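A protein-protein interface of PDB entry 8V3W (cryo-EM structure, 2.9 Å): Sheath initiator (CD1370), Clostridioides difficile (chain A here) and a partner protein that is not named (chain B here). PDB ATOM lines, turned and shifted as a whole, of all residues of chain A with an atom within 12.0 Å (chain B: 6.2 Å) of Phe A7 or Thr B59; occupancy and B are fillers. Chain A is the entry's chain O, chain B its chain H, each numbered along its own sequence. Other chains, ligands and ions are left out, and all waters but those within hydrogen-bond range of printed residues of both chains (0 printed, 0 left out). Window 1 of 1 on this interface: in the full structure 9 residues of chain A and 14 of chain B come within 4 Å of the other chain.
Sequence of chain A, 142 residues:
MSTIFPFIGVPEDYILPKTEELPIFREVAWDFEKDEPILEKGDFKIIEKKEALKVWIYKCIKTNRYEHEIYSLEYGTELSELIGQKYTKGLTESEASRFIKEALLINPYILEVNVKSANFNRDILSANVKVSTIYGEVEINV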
ATOM      1  N   THR A   3       7.712  -2.402  20.897  1.00  0.00           N
ATOM      2  CA  THR A   3       7.363  -2.910  19.580  1.00  0.00           C
ATOM      3  C   THR A   3       6.358  -1.987  18.904  1.00  0.00           C
ATOM      4  O   THR A   3       5.441  -1.469  19.545  1.00  0.00           O
ATOM      5  CB  THR A   3       6.787  -4.319  19.684  1.00  0.00           C
ATOM      6  OG1 THR A   3       5.711  -4.326  20.628  1.00  0.00           O
ATOM      7  CG2 THR A   3       7.858  -5.294  20.147  1.00  0.00           C
ATOM      8  N   ILE A   4       6.540  -1.789  17.600  1.00  0.00           N
ATOM      9  CA  ILE A   4       5.676  -0.895  16.843  1.00  0.00           C
ATOM     10  C   ILE A   4       4.324  -1.555  16.593  1.00  0.00           C
ATOM     11  O   ILE A   4       4.185  -2.779  16.591  1.00  0.00           O
ATOM     12  CB  ILE A   4       6.347  -0.481  15.523  1.00  0.00           C
ATOM     13  CG1 ILE A   4       6.495  -1.691  14.605  1.00  0.00           C
ATOM     14  CG2 ILE A   4       7.705   0.130  15.789  1.00  0.00           C
ATOM     15  CD1 ILE A   4       6.982  -1.348  13.228  1.00  0.00           C
ATOM     16  N   PHE A   5       3.311  -0.720  16.388  1.00  0.00           N
ATOM     17  CA  PHE A   5       1.970  -1.176  16.041  1.00  0.00           C
ATOM     18  C   PHE A   5       1.672  -0.736  14.616  1.00  0.00           C
ATOM     19  O   PHE A   5       1.386   0.449  14.389  1.00  0.00           O
ATOM     20  CB  PHE A   5       0.937  -0.601  17.010  1.00  0.00           C
ATOM     21  CG  PHE A   5      -0.384  -1.311  16.986  1.00  0.00           C
ATOM     22  CD1 PHE A   5      -0.507  -2.587  17.496  1.00  0.00           C
ATOM     23  CD2 PHE A   5      -1.508  -0.692  16.468  1.00  0.00           C
ATOM     24  CE1 PHE A   5      -1.721  -3.238  17.480  1.00  0.00           C
ATOM     25  CE2 PHE A   5      -2.724  -1.339  16.451  1.00  0.00           C
ATOM     26  CZ  PHE A   5      -2.829  -2.615  16.958  1.00  0.00           C
ATOM     27  N   PRO A   6       1.715  -1.632  13.633  1.00  0.00           N
ATOM     28  CA  PRO A   6       1.687  -1.192  12.233  1.00  0.00           C
ATOM     29  C   PRO A   6       0.291  -1.008  11.664  1.00  0.00           C
ATOM     30  O   PRO A   6       0.127  -0.953  10.444  1.00  0.00           O
ATOM     31  CB  PRO A   6       2.434  -2.315  11.503  1.00  0.00           C
ATOM     32  CG  PRO A   6       2.433  -3.495  12.452  1.00  0.00           C
ATOM     33  CD  PRO A   6       1.798  -3.094  13.746  1.00  0.00           C
ATOM     34  N   PHE A   7      -0.719  -0.920  12.518  1.00  0.00           N
ATOM     35  CA  PHE A   7      -2.093  -0.767  12.073  1.00  0.00           C
ATOM     36  C   PHE A   7      -2.649   0.579  12.510  1.00  0.00           C
ATOM     37  O   PHE A   7      -2.130   1.228  13.420  1.00  0.00           O
ATOM     38  CB  PHE A   7      -2.968  -1.906  12.602  1.00  0.00           C
ATOM     39  CG  PHE A   7      -2.384  -3.267  12.378  1.00  0.00           C
ATOM     40  CD1 PHE A   7      -2.395  -3.838  11.119  1.00  0.00           C
ATOM     41  CD2 PHE A   7      -1.815  -3.971  13.419  1.00  0.00           C
ATOM     42  CE1 PHE A   7      -1.858  -5.086  10.906  1.00  0.00           C
ATOM     43  CE2 PHE A   7      -1.276  -5.221  13.211  1.00  0.00           C
ATOM     44  CZ  PHE A   7      -1.298  -5.778  11.953  1.00  0.00           C
ATOM     45  N   ILE A   8      -3.715   1.000  11.832  1.00  0.00           N
ATOM     46  CA  ILE A   8      -4.305   2.305  12.091  1.00  0.00           C
ATOM     47  C   ILE A   8      -5.087   2.264  13.394  1.00  0.00           C
ATOM     48  O   ILE A   8      -5.968   1.418  13.584  1.00  0.00           O
ATOM     49  CB  ILE A   8      -5.197   2.735  10.919  1.00  0.00           C
ATOM     50  CG1 ILE A   8      -4.337   3.031   9.691  1.00  0.00           C
ATOM     51  CG2 ILE A   8      -6.042   3.932  11.308  1.00  0.00           C
ATOM     52  CD1 ILE A   8      -4.956   3.995   8.728  1.00  0.00           C
ATOM     53  N   GLY A   9      -4.767   3.185  14.299  1.00  0.00           N
ATOM     54  CA  GLY A   9      -5.471   3.287  15.558  1.00  0.00           C
ATOM     55  C   GLY A   9      -4.690   2.726  16.724  1.00  0.00           C
ATOM     56  O   GLY A   9      -3.466   2.859  16.783  1.00  0.00           O
ATOM     57  N   VAL A  10      -5.393   2.089  17.654  1.00  0.00           N
ATOM     58  CA  VAL A  10      -4.784   1.508  18.848  1.00  0.00           C
ATOM     59  C   VAL A  10      -5.362   0.121  19.065  1.00  0.00           C
ATOM     60  O   VAL A  10      -6.454  -0.196  18.575  1.00  0.00           O
ATOM     61  CB  VAL A  10      -5.022   2.384  20.095  1.00  0.00           C
ATOM     62  CG1 VAL A  10      -4.030   3.535  20.126  1.00  0.00           C
ATOM     63  CG2 VAL A  10      -6.448   2.898  20.118  1.00  0.00           C
ATOM     64  N   PRO A  11      -4.647  -0.735  19.802  1.00  0.00           N
ATOM     65  CA  PRO A  11      -5.141  -2.105  20.022  1.00  0.00           C
ATOM     66  C   PRO A  11      -6.548  -2.183  20.587  1.00  0.00           C
ATOM     67  O   PRO A  11      -7.206  -3.216  20.418  1.00  0.00           O
ATOM     68  CB  PRO A  11      -4.120  -2.684  21.009  1.00  0.00           C
ATOM     69  CG  PRO A  11      -2.875  -1.945  20.718  1.00  0.00           C
ATOM     70  CD  PRO A  11      -3.278  -0.560  20.321  1.00  0.00           C
ATOM     71  N   GLU A  12      -7.033  -1.133  21.251  1.00  0.00           N
ATOM     72  CA  GLU A  12      -8.365  -1.176  21.843  1.00  0.00           C
ATOM     73  C   GLU A  12      -9.464  -1.204  20.788  1.00  0.00           C
ATOM     74  O   GLU A  12     -10.529  -1.784  21.024  1.00  0.00           O
ATOM     75  CB  GLU A  12      -8.560   0.020  22.775  1.00  0.00           C
ATOM     76  CG  GLU A  12      -7.988  -0.177  24.166  1.00  0.00           C
ATOM     77  CD  GLU A  12      -6.481  -0.338  24.160  1.00  0.00           C
ATOM     78  OE1 GLU A  12      -5.782   0.574  23.672  1.00  0.00           O
ATOM     79  OE2 GLU A  12      -5.996  -1.383  24.643  1.00  0.00           O
ATOM     80  N   ASP A  13      -9.234  -0.583  19.631  1.00  0.00           N
ATOM     81  CA  ASP A  13     -10.266  -0.514  18.603  1.00  0.00           C
ATOM     82  C   ASP A  13     -10.502  -1.844  17.903  1.00  0.00           C
ATOM     83  O   ASP A  13     -11.478  -1.964  17.156  1.00  0.00           O
ATOM     84  CB  ASP A  13      -9.901   0.544  17.564  1.00  0.00           C
ATOM     85  CG  ASP A  13      -9.503   1.857  18.188  1.00  0.00           C
ATOM     86  OD1 ASP A  13      -9.545   1.964  19.430  1.00  0.00           O
ATOM     87  OD2 ASP A  13      -9.151   2.791  17.439  1.00  0.00           O
ATOM     88  N   TYR A  14      -9.641  -2.833  18.110  1.00  0.00           N
ATOM     89  CA  TYR A  14      -9.744  -4.107  17.420  1.00  0.00           C
ATOM     90  C   TYR A  14     -10.383  -5.189  18.272  1.00  0.00           C
ATOM     91  O   TYR A  14     -10.340  -6.364  17.897  1.00  0.00           O
ATOM     92  CB  TYR A  14      -8.361  -4.543  16.937  1.00  0.00           C
ATOM     93  CG  TYR A  14      -7.825  -3.637  15.860  1.00  0.00           C
ATOM     94  CD1 TYR A  14      -8.218  -3.793  14.544  1.00  0.00           C
ATOM     95  CD2 TYR A  14      -6.971  -2.594  16.169  1.00  0.00           C
ATOM     96  CE1 TYR A  14      -7.747  -2.961  13.559  1.00  0.00           C
ATOM     97  CE2 TYR A  14      -6.496  -1.751  15.189  1.00  0.00           C
ATOM     98  CZ  TYR A  14      -6.887  -1.940  13.888  1.00  0.00           C
ATOM     99  OH  TYR A  14      -6.416  -1.104  12.909  1.00  0.00           O
ATOM    100  N   ILE A  15     -10.970  -4.827  19.404  1.00  0.00           N
ATOM    101  CA  ILE A  15     -11.711  -5.773  20.227  1.00  0.00           C
ATOM    102  C   ILE A  15     -13.160  -5.750  19.763  1.00  0.00           C
ATOM    103  O   ILE A  15     -13.829  -4.713  19.831  1.00  0.00           O
ATOM    104  CB  ILE A  15     -11.595  -5.438  21.724  1.00  0.00           C
ATOM    105  CG1 ILE A  15     -10.336  -6.051  22.353  1.00  0.00           C
ATOM    106  CG2 ILE A  15     -12.816  -5.934  22.480  1.00  0.00           C
ATOM    107  CD1 ILE A  15      -9.055  -5.896  21.567  1.00  0.00           C
ATOM    108  N   TRP B   5     -14.278  -5.522   7.800  1.00  0.00           N
ATOM    109  CA  TRP B   5     -14.281  -4.219   8.446  1.00  0.00           C
ATOM    110  C   TRP B   5     -13.062  -3.429   7.994  1.00  0.00           C
ATOM    111  O   TRP B   5     -11.991  -4.000   7.780  1.00  0.00           O
ATOM    112  CB  TRP B   5     -14.272  -4.353   9.968  1.00  0.00           C
ATOM    113  CG  TRP B   5     -15.515  -4.952  10.528  1.00  0.00           C
ATOM    114  CD1 TRP B   5     -15.901  -6.251  10.440  1.00  0.00           C
ATOM    115  CD2 TRP B   5     -16.535  -4.278  11.267  1.00  0.00           C
ATOM    116  NE1 TRP B   5     -17.101  -6.433  11.076  1.00  0.00           N
ATOM    117  CE2 TRP B   5     -17.512  -5.234  11.594  1.00  0.00           C
ATOM    118  CE3 TRP B   5     -16.718  -2.958  11.686  1.00  0.00           C
ATOM    119  CZ2 TRP B   5     -18.654  -4.915  12.315  1.00  0.00           C
ATOM    120  CZ3 TRP B   5     -17.851  -2.644  12.402  1.00  0.00           C
ATOM    121  CH2 TRP B   5     -18.805  -3.618  12.710  1.00  0.00           C
ATOM    122  N   VAL B   6     -13.222  -2.116   7.857  1.00  0.00           N
ATOM    123  CA  VAL B   6     -12.161  -1.237   7.386  1.00  0.00           C
ATOM    124  C   VAL B   6     -11.985  -0.093   8.376  1.00  0.00           C
ATOM    125  O   VAL B   6     -12.966   0.540   8.778  1.00  0.00           O
ATOM    126  CB  VAL B   6     -12.463  -0.693   5.977  1.00  0.00           C
ATOM    127  CG1 VAL B   6     -11.472   0.371   5.603  1.00  0.00           C
ATOM    128  CG2 VAL B   6     -12.415  -1.814   4.965  1.00  0.00           C
ATOM    129  N   HIS B   7     -10.741   0.170   8.762  1.00  0.00           N
ATOM    130  CA  HIS B   7     -10.388   1.263   9.658  1.00  0.00           C
ATOM    131  C   HIS B   7      -9.726   2.375   8.855  1.00  0.00           C
ATOM    132  O   HIS B   7      -8.737   2.134   8.161  1.00  0.00           O
ATOM    133  CB  HIS B   7      -9.441   0.781  10.758  1.00  0.00           C
ATOM    134  CG  HIS B   7     -10.076  -0.139  11.753  1.00  0.00           C
ATOM    135  ND1 HIS B   7     -10.728  -1.295  11.387  1.00  0.00           N
ATOM    136  CD2 HIS B   7     -10.139  -0.085  13.103  1.00  0.00           C
ATOM    137  CE1 HIS B   7     -11.176  -1.907  12.467  1.00  0.00           C
ATOM    138  NE2 HIS B   7     -10.830  -1.194  13.522  1.00  0.00           N
ATOM    139  N   ILE B   8     -10.262   3.590   8.957  1.00  0.00           N
ATOM    140  CA  ILE B   8      -9.751   4.733   8.213  1.00  0.00           C
ATOM    141  C   ILE B   8      -8.898   5.583   9.144  1.00  0.00           C
ATOM    142  O   ILE B   8      -8.989   5.495  10.371  1.00  0.00           O
ATOM    143  CB  ILE B   8     -10.892   5.563   7.579  1.00  0.00           C
ATOM    144  CG1 ILE B   8     -11.921   4.648   6.929  1.00  0.00           C
ATOM    145  CG2 ILE B   8     -10.360   6.502   6.517  1.00  0.00           C
ATOM    146  CD1 ILE B   8     -11.425   3.969   5.696  1.00  0.00           C
ATOM    147  N   ALA B  57      -3.369   2.431   2.388  1.00  0.00           N
ATOM    148  CA  ALA B  57      -2.713   2.218   3.679  1.00  0.00           C
ATOM    149  C   ALA B  57      -3.695   2.374   4.840  1.00  0.00           C
ATOM    150  O   ALA B  57      -3.394   3.001   5.853  1.00  0.00           O
ATOM    151  CB  ALA B  57      -1.505   3.142   3.851  1.00  0.00           C
ATOM    152  N   SER B  58      -4.871   1.779   4.688  1.00  0.00           N
ATOM    153  CA  SER B  58      -5.843   1.657   5.759  1.00  0.00           C
ATOM    154  C   SER B  58      -6.061   0.181   6.057  1.00  0.00           C
ATOM    155  O   SER B  58      -5.937  -0.668   5.172  1.00  0.00           O
ATOM    156  CB  SER B  58      -7.167   2.331   5.398  1.00  0.00           C
ATOM    157  OG  SER B  58      -7.562   2.012   4.084  1.00  0.00           O
ATOM    158  N   THR B  59      -6.373  -0.123   7.311  1.00  0.00           N
ATOM    159  CA  THR B  59      -6.418  -1.506   7.763  1.00  0.00           C
ATOM    160  C   THR B  59      -7.746  -2.164   7.418  1.00  0.00           C
ATOM    161  O   THR B  59      -8.810  -1.550   7.530  1.00  0.00           O
ATOM    162  CB  THR B  59      -6.181  -1.573   9.268  1.00  0.00           C
ATOM    163  OG1 THR B  59      -5.002  -0.829   9.590  1.00  0.00           O
ATOM    164  CG2 THR B  59      -5.988  -3.004   9.708  1.00  0.00           C
ATOM    165  N   VAL B  60      -7.677  -3.426   7.004  1.00  0.00           N
ATOM    166  CA  VAL B  60      -8.848  -4.226   6.670  1.00  0.00           C
ATOM    167  C   VAL B  60      -8.794  -5.526   7.462  1.00  0.00           C
ATOM    168  O   VAL B  60      -7.740  -6.163   7.555  1.00  0.00           O
ATOM    169  CB  VAL B  60      -8.929  -4.496   5.153  1.00  0.00           C
ATOM    170  CG1 VAL B  60      -7.592  -4.968   4.623  1.00  0.00           C
ATOM    171  CG2 VAL B  60     -10.012  -5.501   4.843  1.00  0.00           C
ATOM    172  N   CYS B  61      -9.930  -5.911   8.046  1.00  0.00           N
ATOM    173  CA  CYS B  61     -10.039  -7.088   8.898  1.00  0.00           C
ATOM    174  C   CYS B  61     -11.042  -8.067   8.307  1.00  0.00           C
ATOM    175  O   CYS B  61     -12.115  -7.667   7.851  1.00  0.00           O
ATOM    176  CB  CYS B  61     -10.471  -6.704  10.314  1.00  0.00           C
ATOM    177  SG  CYS B  61      -9.255  -5.784  11.258  1.00  0.00           S
ATOM    178  N   ARG B  71      -5.492  -9.641   8.958  1.00  0.00           N
ATOM    179  CA  ARG B  71      -5.426  -8.213   9.242  1.00  0.00           C
ATOM    180  C   ARG B  71      -4.245  -7.647   8.474  1.00  0.00           C
ATOM    181  O   ARG B  71      -3.116  -8.103   8.662  1.00  0.00           O
ATOM    182  CB  ARG B  71      -5.274  -7.943  10.738  1.00  0.00           C
ATOM    183  CG  ARG B  71      -5.549  -6.504  11.120  1.00  0.00           C
ATOM    184  CD  ARG B  71      -5.224  -6.221  12.571  1.00  0.00           C
ATOM    185  NE  ARG B  71      -5.974  -7.070  13.485  1.00  0.00           N
ATOM    186  CZ  ARG B  71      -5.867  -7.023  14.805  1.00  0.00           C
ATOM    187  NH1 ARG B  71      -5.037  -6.185  15.400  1.00  0.00           N
ATOM    188  NH2 ARG B  71      -6.614  -7.836  15.545  1.00  0.00           N
ATOM    189  N   GLY B  72      -4.493  -6.657   7.621  1.00  0.00           N
ATOM    190  CA  GLY B  72      -3.418  -6.175   6.777  1.00  0.00           C
ATOM    191  C   GLY B  72      -3.674  -4.789   6.232  1.00  0.00           C
ATOM    192  O   GLY B  72      -4.701  -4.164   6.498  1.00  0.00           O
ATOM    193  N   MET B  73      -2.710  -4.322   5.448  1.00  0.00           N
ATOM    194  CA  MET B  73      -2.696  -2.984   4.881  1.00  0.00           C
ATOM    195  C   MET B  73      -3.116  -3.012   3.417  1.00  0.00           C
ATOM    196  O   MET B  73      -2.830  -3.965   2.691  1.00  0.00           O
ATOM    197  CB  MET B  73      -1.302  -2.372   5.004  1.00  0.00           C
ATOM    198  CG  MET B  73      -1.260  -0.872   4.856  1.00  0.00           C
ATOM    199  SD  MET B  73       0.319  -0.145   5.330  1.00  0.00           S
ATOM    200  CE  MET B  73       1.102  -1.538   6.123  1.00  0.00           C
ATOM    201  N   ILE B  74      -3.791  -1.952   2.991  1.00  0.00           N
ATOM    202  CA  ILE B  74      -4.215  -1.809   1.603  1.00  0.00           C
ATOM    203  C   ILE B  74      -3.075  -1.205   0.794  1.00  0.00           C
ATOM    204  O   ILE B  74      -2.495  -0.187   1.182  1.00  0.00           O
ATOM    205  CB  ILE B  74      -5.484  -0.951   1.518  1.00  0.00           C
ATOM    206  CG1 ILE B  74      -6.656  -1.703   2.148  1.00  0.00           C
ATOM    207  CG2 ILE B  74      -5.786  -0.571   0.087  1.00  0.00           C
ATOM    208  CD1 ILE B  74      -7.989  -1.093   1.878  1.00  0.00           C
ATOM    209  N   MET B  93       1.160  -8.360   7.397  1.00  0.00           N
ATOM    210  CA  MET B  93       2.231  -7.584   8.009  1.00  0.00           C
ATOM    211  C   MET B  93       3.607  -8.177   7.724  1.00  0.00           C
ATOM    212  O   MET B  93       4.617  -7.492   7.912  1.00  0.00           O
ATOM    213  CB  MET B  93       1.972  -7.472   9.518  1.00  0.00           C
ATOM    214  CG  MET B  93       3.156  -7.060  10.376  1.00  0.00           C
ATOM    215  SD  MET B  93       2.836  -7.106  12.147  1.00  0.00           S
ATOM    216  CE  MET B  93       2.090  -8.719  12.304  1.00  0.00           C
ATOM    217  N   LEU B 170      -2.215 -12.142  12.714  1.00  0.00           N
ATOM    218  CA  LEU B 170      -2.737 -10.907  13.308  1.00  0.00           C
ATOM    219  C   LEU B 170      -1.549 -10.007  13.623  1.00  0.00           C
ATOM    220  O   LEU B 170      -0.866  -9.579  12.679  1.00  0.00           O
ATOM    221  CB  LEU B 170      -3.656 -11.245  14.481  1.00  0.00           C
ATOM    222  CG  LEU B 170      -4.863 -12.119  14.138  1.00  0.00           C
ATOM    223  CD1 LEU B 170      -5.880 -12.066  15.250  1.00  0.00           C
ATOM    224  CD2 LEU B 170      -5.495 -11.687  12.827  1.00  0.00           C
ATOM    225  N   ASP B 171      -1.260  -9.692  14.886  1.00  0.00           N
ATOM    226  CA  ASP B 171      -0.172  -8.790  15.233  1.00  0.00           C
ATOM    227  C   ASP B 171       1.062  -9.516  15.766  1.00  0.00           C
ATOM    228  O   ASP B 171       1.941  -8.874  16.346  1.00  0.00           O
ATOM    229  CB  ASP B 171      -0.650  -7.759  16.253  1.00  0.00           C
ATOM    230  CG  ASP B 171      -1.602  -8.347  17.273  1.00  0.00           C
ATOM    231  OD1 ASP B 171      -1.667  -9.586  17.386  1.00  0.00           O
ATOM    232  OD2 ASP B 171      -2.287  -7.567  17.965  1.00  0.00           O
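Among the printed residues, pairs that only touch across the chains: Ile A8 with Ala B57 (3.4 Å), Ile A8 with Ile B8 (3.5 Å), Tyr A14 with His B7 (3.6 Å), Tyr A14 with Thr B59 (3.6 Å), Pro A6 with Met B93 (3.6 Å), Asp A13 with His B7 (3.8 Å), Phe A7 with Thr B59 (3.8 Å), Tyr A14 with Arg B71 (3.8 Å), Ile A8 with Ser B58 (3.9 Å), Phe A7 with Leu B170 (3.9 Å), Phe A7 with Arg B71 (3.9 Å) and Tyr A14 with Cys B61 (3.9 Å).
The backbone carbonyl oxygen (O) of Ile A8 lies within hydrogen-bond range of the side-chain hydroxyl (OH) of Tyr A14 (2.6 Å). N of Cys B61 is in hydrogen-bond range of O of Trp B5 (2.8 Å). The backbone NH of His B7 sits at hydrogen-bond distance from the backbone carbonyl oxygen of Thr B59 (2.9 Å). The backbone carbonyl oxygen (O) of Ile B74 is in hydrogen-bond range of the backbone NH (N) of Ala B57. O of Ser B58 lies close to N of Ile B74.
Phe A5 touches none of the printed residues of chain B. Printed residues of chain B within 4 Å of Pro A6: Met B93 (3.6 Å). Printed residues of chain B within 4 Å of Phe A7: Thr B59 (3.8 Å), Arg B71 (3.9 Å) and Leu B170 (3.9 Å). Of the printed residues of chain B, Ile A8 touches Ile B8 (3.5 Å), Ala B57 (3.4 Å), Ser B58 (3.9 Å) and Thr B59 (3.2 Å). Val A10 touches none of the printed residues of chain B. Of the printed residues of chain B, Asp A13 touches His B7. Of the printed residues of chain B, Tyr A14 touches His B7, Thr B59, Cys B61 and Arg B71. No residue of chain A comes within 4 Å of Val B6. Of chain A, only Ile A8 comes within 4 Å of Ala B57. Thr B59 touches three residues of chain A. No residue of chain A comes within 4 Å of Val B60. Cys B61 touches one residue of chain A. No residue of chain A comes within 4 Å of Met B73. No residue of chain A comes within 4 Å of Ile B74. Of chain A, only Pro A6 (3.6 Å) comes within 4 Å of Met B93. Of the printed residues of chain A, Leu B170 touches Phe A7. The nearest residue of chain A that does not touch Thr B59 is Pro A6 (5.2 Å). The nearest printed residue of chain A that does not touch Leu B170 is Pro A6 (6.9 Å).
Hydrophobic or aromatic side chains of chain A that line the printed part of chain B: Pro A6, Phe A7, Ile A8 and Tyr A14. Of the 16 printed residues of chain B, 9 touch a printed residue of chain A. Hydrophobic or aromatic side chains of chain B within 4 Å of the printed part of chain A: His B7 and Met B93. Among the printed residues, no Asp or Glu carboxylate lies within 4 Å of a Lys or Arg side-chain nitrogen of the other chain.
The side-chain hydroxyl of Thr B59 lies within hydrogen-bond range of the backbone NH of Ile A8 (3.2 Å).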
